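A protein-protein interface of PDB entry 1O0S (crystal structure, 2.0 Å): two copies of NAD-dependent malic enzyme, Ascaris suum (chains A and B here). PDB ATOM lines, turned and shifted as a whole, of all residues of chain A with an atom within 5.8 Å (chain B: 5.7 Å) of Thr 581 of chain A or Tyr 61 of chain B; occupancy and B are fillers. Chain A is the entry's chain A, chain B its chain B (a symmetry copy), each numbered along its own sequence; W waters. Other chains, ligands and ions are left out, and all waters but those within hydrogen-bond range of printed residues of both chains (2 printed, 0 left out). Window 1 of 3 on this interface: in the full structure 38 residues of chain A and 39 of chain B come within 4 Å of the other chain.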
ATOM      1  N   SER A   2      30.076  30.942  13.168  1.00  0.00           N
ATOM      2  CA  SER A   2      30.292  30.213  11.884  1.00  0.00           C
ATOM      3  C   SER A   2      31.605  30.630  11.227  1.00  0.00           C
ATOM      4  O   SER A   2      32.153  31.693  11.511  1.00  0.00           O
ATOM      5  CB  SER A   2      29.135  30.477  10.907  1.00  0.00           C
ATOM      6  OG  SER A   2      29.219  31.773  10.340  1.00  0.00           O
ATOM      7  N   VAL A   3      32.099  29.784  10.336  1.00  0.00           N
ATOM      8  CA  VAL A   3      33.349  30.042   9.643  1.00  0.00           C
ATOM      9  C   VAL A   3      33.168  30.991   8.451  1.00  0.00           C
ATOM     10  O   VAL A   3      32.089  31.062   7.861  1.00  0.00           O
ATOM     11  CB  VAL A   3      33.956  28.697   9.195  1.00  0.00           C
ATOM     12  CG1 VAL A   3      34.982  28.907   8.118  1.00  0.00           C
ATOM     13  CG2 VAL A   3      34.577  27.996  10.410  1.00  0.00           C
ATOM     14  N   VAL A   9      35.706  24.206   7.365  1.00  0.00           N
ATOM     15  CA  VAL A   9      35.195  23.956   8.707  1.00  0.00           C
ATOM     16  C   VAL A   9      36.314  23.342   9.548  1.00  0.00           C
ATOM     17  O   VAL A   9      37.221  22.697   9.009  1.00  0.00           O
ATOM     18  CB  VAL A   9      33.975  23.002   8.684  1.00  0.00           C
ATOM     19  CG1 VAL A   9      32.791  23.701   8.034  1.00  0.00           C
ATOM     20  CG2 VAL A   9      34.311  21.733   7.925  1.00  0.00           C
ATOM     21  N   THR A  34      27.955  14.169  13.744  1.00  0.00           N
ATOM     22  CA  THR A  34      26.927  14.687  14.644  1.00  0.00           C
ATOM     23  C   THR A  34      25.881  13.631  14.997  1.00  0.00           C
ATOM     24  O   THR A  34      25.327  12.975  14.118  1.00  0.00           O
ATOM     25  CB  THR A  34      26.250  15.921  14.011  1.00  0.00           C
ATOM     26  OG1 THR A  34      27.213  16.980  13.912  1.00  0.00           O
ATOM     27  CG2 THR A  34      25.065  16.392  14.840  1.00  0.00           C
ATOM     28  N   TYR A  61      22.139  23.340  24.035  1.00  0.00           N
ATOM     29  CA  TYR A  61      21.880  22.997  22.637  1.00  0.00           C
ATOM     30  C   TYR A  61      21.374  21.576  22.450  1.00  0.00           C
ATOM     31  O   TYR A  61      20.411  21.345  21.714  1.00  0.00           O
ATOM     32  CB  TYR A  61      23.147  23.151  21.788  1.00  0.00           C
ATOM     33  CG  TYR A  61      23.417  24.545  21.276  1.00  0.00           C
ATOM     34  CD1 TYR A  61      24.596  25.224  21.619  1.00  0.00           C
ATOM     35  CD2 TYR A  61      22.525  25.171  20.403  1.00  0.00           C
ATOM     36  CE1 TYR A  61      24.883  26.497  21.094  1.00  0.00           C
ATOM     37  CE2 TYR A  61      22.798  26.435  19.877  1.00  0.00           C
ATOM     38  CZ  TYR A  61      23.975  27.090  20.223  1.00  0.00           C
ATOM     39  OH  TYR A  61      24.232  28.325  19.686  1.00  0.00           O
ATOM     40  N   ILE A 578      28.361  19.086  17.827  1.00  0.00           N
ATOM     41  CA  ILE A 578      27.499  20.013  17.105  1.00  0.00           C
ATOM     42  C   ILE A 578      28.066  20.349  15.727  1.00  0.00           C
ATOM     43  O   ILE A 578      29.266  20.625  15.590  1.00  0.00           O
ATOM     44  CB  ILE A 578      27.334  21.298  17.917  1.00  0.00           C
ATOM     45  CG1 ILE A 578      26.581  20.971  19.208  1.00  0.00           C
ATOM     46  CG2 ILE A 578      26.628  22.367  17.092  1.00  0.00           C
ATOM     47  CD1 ILE A 578      26.601  22.086  20.234  1.00  0.00           C
ATOM     48  N   ASN A 579      27.208  20.318  14.708  1.00  0.00           N
ATOM     49  CA  ASN A 579      27.637  20.618  13.345  1.00  0.00           C
ATOM     50  C   ASN A 579      28.394  21.933  13.271  1.00  0.00           C
ATOM     51  O   ASN A 579      28.035  22.912  13.935  1.00  0.00           O
ATOM     52  CB  ASN A 579      26.441  20.734  12.389  1.00  0.00           C
ATOM     53  CG  ASN A 579      25.825  19.404  12.043  1.00  0.00           C
ATOM     54  OD1 ASN A 579      24.911  18.936  12.721  1.00  0.00           O
ATOM     55  ND2 ASN A 579      26.319  18.782  10.977  1.00  0.00           N
ATOM     56  N   ALA A 580      29.442  21.961  12.460  1.00  0.00           N
ATOM     57  CA  ALA A 580      30.191  23.193  12.271  1.00  0.00           C
ATOM     58  C   ALA A 580      29.385  23.960  11.224  1.00  0.00           C
ATOM     59  O   ALA A 580      28.845  23.357  10.295  1.00  0.00           O
ATOM     60  CB  ALA A 580      31.594  22.893  11.746  1.00  0.00           C
ATOM     61  N   THR A 581      29.275  25.273  11.393  1.00  0.00           N
ATOM     62  CA  THR A 581      28.541  26.118  10.448  1.00  0.00           C
ATOM     63  C   THR A 581      29.554  26.916   9.642  1.00  0.00           C
ATOM     64  O   THR A 581      30.669  27.161  10.102  1.00  0.00           O
ATOM     65  CB  THR A 581      27.611  27.113  11.172  1.00  0.00           C
ATOM     66  OG1 THR A 581      28.376  27.858  12.128  1.00  0.00           O
ATOM     67  CG2 THR A 581      26.478  26.376  11.891  1.00  0.00           C
ATOM     68  N   TYR A 582      29.176  27.318   8.437  1.00  0.00           N
ATOM     69  CA  TYR A 582      30.089  28.081   7.601  1.00  0.00           C
ATOM     70  C   TYR A 582      29.337  28.935   6.590  1.00  0.00           C
ATOM     71  O   TYR A 582      28.262  28.563   6.104  1.00  0.00           O
ATOM     72  CB  TYR A 582      31.073  27.143   6.895  1.00  0.00           C
ATOM     73  CG  TYR A 582      30.438  26.150   5.947  1.00  0.00           C
ATOM     74  CD1 TYR A 582      30.147  26.502   4.628  1.00  0.00           C
ATOM     75  CD2 TYR A 582      30.142  24.851   6.361  1.00  0.00           C
ATOM     76  CE1 TYR A 582      29.583  25.582   3.741  1.00  0.00           C
ATOM     77  CE2 TYR A 582      29.570  23.918   5.481  1.00  0.00           C
ATOM     78  CZ  TYR A 582      29.298  24.291   4.171  1.00  0.00           C
ATOM     79  OH  TYR A 582      28.762  23.363   3.293  1.00  0.00           O
ATOM     80  N   ASP A 583      29.917  30.092   6.299  1.00  0.00           N
ATOM     81  CA  ASP A 583      29.333  31.044   5.378  1.00  0.00           C
ATOM     82  C   ASP A 583      29.461  30.686   3.918  1.00  0.00           C
ATOM     83  O   ASP A 583      30.337  29.929   3.506  1.00  0.00           O
ATOM     84  CB  ASP A 583      29.959  32.423   5.575  1.00  0.00           C
ATOM     85  CG  ASP A 583      29.623  33.020   6.907  1.00  0.00           C
ATOM     86  OD1 ASP A 583      28.527  32.721   7.398  1.00  0.00           O
ATOM     87  OD2 ASP A 583      30.437  33.795   7.456  1.00  0.00           O
ATOM     88  N   ARG B  38      16.126  15.099  12.455  1.00  0.00           N
ATOM     89  CA  ARG B  38      17.164  15.783  11.694  1.00  0.00           C
ATOM     90  C   ARG B  38      17.073  15.329  10.242  1.00  0.00           C
ATOM     91  O   ARG B  38      16.375  14.366   9.928  1.00  0.00           O
ATOM     92  CB  ARG B  38      18.557  15.410  12.230  1.00  0.00           C
ATOM     93  CG  ARG B  38      18.906  15.953  13.618  1.00  0.00           C
ATOM     94  CD  ARG B  38      20.236  15.344  14.105  1.00  0.00           C
ATOM     95  NE  ARG B  38      21.345  15.572  13.179  1.00  0.00           N
ATOM     96  CZ  ARG B  38      21.948  16.749  13.006  1.00  0.00           C
ATOM     97  NH1 ARG B  38      21.554  17.807  13.698  1.00  0.00           N
ATOM     98  NH2 ARG B  38      22.955  16.871  12.151  1.00  0.00           N
ATOM     99  N   LEU B  56      20.713  29.026   5.771  1.00  0.00           N
ATOM    100  CA  LEU B  56      21.889  28.181   5.578  1.00  0.00           C
ATOM    101  C   LEU B  56      22.394  27.608   6.911  1.00  0.00           C
ATOM    102  O   LEU B  56      22.779  26.443   6.991  1.00  0.00           O
ATOM    103  CB  LEU B  56      23.022  28.972   4.916  1.00  0.00           C
ATOM    104  CG  LEU B  56      24.315  28.176   4.773  1.00  0.00           C
ATOM    105  CD1 LEU B  56      24.104  27.007   3.820  1.00  0.00           C
ATOM    106  CD2 LEU B  56      25.412  29.094   4.257  1.00  0.00           C
ATOM    107  N   TYR B  57      22.403  28.433   7.953  1.00  0.00           N
ATOM    108  CA  TYR B  57      22.858  27.982   9.259  1.00  0.00           C
ATOM    109  C   TYR B  57      21.940  26.904   9.813  1.00  0.00           C
ATOM    110  O   TYR B  57      22.412  25.922  10.370  1.00  0.00           O
ATOM    111  CB  TYR B  57      22.932  29.162  10.232  1.00  0.00           C
ATOM    112  CG  TYR B  57      23.939  30.209   9.807  1.00  0.00           C
ATOM    113  CD1 TYR B  57      23.641  31.570   9.918  1.00  0.00           C
ATOM    114  CD2 TYR B  57      25.180  29.842   9.258  1.00  0.00           C
ATOM    115  CE1 TYR B  57      24.541  32.538   9.494  1.00  0.00           C
ATOM    116  CE2 TYR B  57      26.089  30.806   8.831  1.00  0.00           C
ATOM    117  CZ  TYR B  57      25.759  32.153   8.951  1.00  0.00           C
ATOM    118  OH  TYR B  57      26.632  33.126   8.529  1.00  0.00           O
ATOM    119  N   GLU B  58      20.631  27.084   9.674  1.00  0.00           N
ATOM    120  CA  GLU B  58      19.698  26.081  10.172  1.00  0.00           C
ATOM    121  C   GLU B  58      19.966  24.748   9.486  1.00  0.00           C
ATOM    122  O   GLU B  58      20.033  23.704  10.140  1.00  0.00           O
ATOM    123  CB  GLU B  58      18.251  26.505   9.900  1.00  0.00           C
ATOM    124  CG  GLU B  58      17.750  27.649  10.765  1.00  0.00           C
ATOM    125  CD  GLU B  58      16.334  28.099  10.397  1.00  0.00           C
ATOM    126  OE1 GLU B  58      15.419  27.964  11.239  1.00  0.00           O
ATOM    127  OE2 GLU B  58      16.137  28.587   9.265  1.00  0.00           O
ATOM    128  N   ARG B  59      20.129  24.785   8.166  1.00  0.00           N
ATOM    129  CA  ARG B  59      20.365  23.572   7.392  1.00  0.00           C
ATOM    130  C   ARG B  59      21.624  22.845   7.846  1.00  0.00           C
ATOM    131  O   ARG B  59      21.646  21.624   7.908  1.00  0.00           O
ATOM    132  CB  ARG B  59      20.475  23.895   5.899  1.00  0.00           C
ATOM    133  CG  ARG B  59      19.243  24.583   5.311  1.00  0.00           C
ATOM    134  CD  ARG B  59      19.422  24.864   3.815  1.00  0.00           C
ATOM    135  NE  ARG B  59      18.378  25.750   3.295  1.00  0.00           N
ATOM    136  CZ  ARG B  59      18.153  25.961   1.999  1.00  0.00           C
ATOM    137  NH1 ARG B  59      18.893  25.349   1.074  1.00  0.00           N
ATOM    138  NH2 ARG B  59      17.184  26.780   1.625  1.00  0.00           N
ATOM    139  N   GLN B  60      22.671  23.601   8.154  1.00  0.00           N
ATOM    140  CA  GLN B  60      23.930  23.013   8.589  1.00  0.00           C
ATOM    141  C   GLN B  60      23.769  22.382   9.971  1.00  0.00           C
ATOM    142  O   GLN B  60      24.137  21.219  10.183  1.00  0.00           O
ATOM    143  CB  GLN B  60      25.021  24.087   8.602  1.00  0.00           C
ATOM    144  CG  GLN B  60      25.178  24.762   7.239  1.00  0.00           C
ATOM    145  CD  GLN B  60      26.292  25.792   7.195  1.00  0.00           C
ATOM    146  OE1 GLN B  60      26.541  26.513   8.169  1.00  0.00           O
ATOM    147  NE2 GLN B  60      26.954  25.879   6.054  1.00  0.00           N
ATOM    148  N   TYR B  61      23.205  23.157  10.894  1.00  0.00           N
ATOM    149  CA  TYR B  61      22.960  22.716  12.272  1.00  0.00           C
ATOM    150  C   TYR B  61      22.059  21.486  12.358  1.00  0.00           C
ATOM    151  O   TYR B  61      22.325  20.558  13.124  1.00  0.00           O
ATOM    152  CB  TYR B  61      22.271  23.828  13.072  1.00  0.00           C
ATOM    153  CG  TYR B  61      23.175  24.853  13.710  1.00  0.00           C
ATOM    154  CD1 TYR B  61      22.854  26.215  13.662  1.00  0.00           C
ATOM    155  CD2 TYR B  61      24.311  24.468  14.423  1.00  0.00           C
ATOM    156  CE1 TYR B  61      23.640  27.172  14.309  1.00  0.00           C
ATOM    157  CE2 TYR B  61      25.107  25.418  15.077  1.00  0.00           C
ATOM    158  CZ  TYR B  61      24.763  26.765  15.015  1.00  0.00           C
ATOM    159  OH  TYR B  61      25.536  27.699  15.658  1.00  0.00           O
ATOM    160  N   LEU B  62      20.980  21.498  11.582  1.00  0.00           N
ATOM    161  CA  LEU B  62      19.995  20.426  11.601  1.00  0.00           C
ATOM    162  C   LEU B  62      20.258  19.278  10.631  1.00  0.00           C
ATOM    163  O   LEU B  62      19.444  18.355  10.527  1.00  0.00           O
ATOM    164  CB  LEU B  62      18.607  21.011  11.341  1.00  0.00           C
ATOM    165  CG  LEU B  62      18.148  22.038  12.384  1.00  0.00           C
ATOM    166  CD1 LEU B  62      16.969  22.820  11.845  1.00  0.00           C
ATOM    167  CD2 LEU B  62      17.778  21.338  13.692  1.00  0.00           C
ATOM    168  N   GLY B  63      21.384  19.326   9.931  1.00  0.00           N
ATOM    169  CA  GLY B  63      21.700  18.258   8.996  1.00  0.00           C
ATOM    170  C   GLY B  63      20.796  18.209   7.774  1.00  0.00           C
ATOM    171  O   GLY B  63      20.514  17.126   7.248  1.00  0.00           O
ATOM    172  N   ILE B 578      15.979  25.570  17.082  1.00  0.00           N
ATOM    173  CA  ILE B 578      17.239  25.363  17.778  1.00  0.00           C
ATOM    174  C   ILE B 578      17.199  26.010  19.148  1.00  0.00           C
ATOM    175  O   ILE B 578      16.730  27.143  19.303  1.00  0.00           O
ATOM    176  CB  ILE B 578      18.390  25.956  16.962  1.00  0.00           C
ATOM    177  CG1 ILE B 578      18.482  25.221  15.631  1.00  0.00           C
ATOM    178  CG2 ILE B 578      19.703  25.771  17.680  1.00  0.00           C
ATOM    179  CD1 ILE B 578      19.446  25.848  14.613  1.00  0.00           C
HETATM  180  O   HOH W   1      24.851  19.631   7.984  1.00  0.00           O
HETATM  181  O   HOH W   2      24.058  20.470  14.965  1.00  0.00           O
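OG of Ser 2 of chain A sits at hydrogen-bond distance from OD1 of Asp 583 of chain A.
N of Val 3 of chain A is in hydrogen-bond range of O of Thr 581 of chain A, at 3.0 Å.
N of Asp 583 of chain A is in hydrogen-bond range of O of Val 3 of chain A, 2.8 Å away.
The side-chain hydroxyl (OG1) of Thr 34 of chain A is in hydrogen-bond range of the side-chain amide oxygen (OD1) of Asn 579 of chain A (3.2 Å).
NH1 of Arg 38 of chain B sits at hydrogen-bond distance from O of Tyr 61 of chain B, 2.9 Å away.
Water W2 lies within hydrogen-bond range of the backbone carbonyl oxygen (O) of Tyr 61 of chain B (2.5 Å) and the side-chain amide oxygen (OD1) of Asn 579 of chain A (2.8 Å).
Water W1 bridges the backbone carbonyl oxygen (O) of Gln 60 of chain B and the side-chain amide nitrogen (ND2) of Asn 579 of chain A.
Printed residues of chain A that touch a printed residue of chain B: Ser 2, Thr 34, Tyr 61, Ile 578, Asn 579, Thr 581, Tyr 582 and Asp 583.
Of the 10 printed residues of chain B, 6 touch a printed residue of chain A.
Hydrophobic or aromatic side chains of chain B that line the printed part of chain A: Leu 56, Tyr 57, Tyr 61 and Ile 578.
Tyr 61 of chain A touches Ile 578 of chain B, and with the chains exchanged Ile 578 of chain A touches Tyr 61 of chain B.
Positions printed for both chains: 61 and 578.
Tyr 61 of chain B touches just these residues of chain A: Ile 578 (3.96 Å), Asn 579 (3.1 Å) and Thr 581 (3.6 Å).
Of the printed residues of chain A, Leu 56 of chain B touches Tyr 582.
Of the printed residues of chain B, Tyr 582 of chain A touches Leu 56 and Gln 60.
Of the printed residues of chain B, Asp 583 of chain A touches Tyr 57.
Thr 34 of chain A touches Arg 38 of chain B.
Ile 578 of chain B touches Tyr 61 of chain A (CG2 to CE2, 3.9 Å).
Tyr 61 of chain B touches Ile 578 of chain A.
Gln 60 of chain B touches Thr 581 of chain A (OE1 to CA, 3.1 Å).
Thr 581 of chain A touches Tyr 61 of chain B (CG2 to CZ, 3.6 Å).
Leu 56 of chain B touches Tyr 582 of chain A.
The side-chain hydroxyl (OG) of Ser 2 of chain A is in hydrogen-bond range of the side-chain hydroxyl (OH) of Tyr 57 of chain B, 3.4 Å away.
OD1 of Asn 579 of chain A sits at hydrogen-bond distance from NH2 of Arg 38 of chain B.
The side-chain amide nitrogen (ND2) of Asn 579 of chain A sits close to the backbone carbonyl oxygen (O) of Gln 60 of chain B.
The side-chain amide oxygen of Asn 579 of chain A lies close to the backbone carbonyl oxygen of Tyr 61 of chain B (3.1 Å).
OE1 of Gln 60 of chain B sits at hydrogen-bond distance from N of Tyr 582 of chain A (2.8 Å).
The side-chain carboxylate (OD1) of Asp 583 of chain A lies close to the side-chain hydroxyl (OH) of Tyr 57 of chain B.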
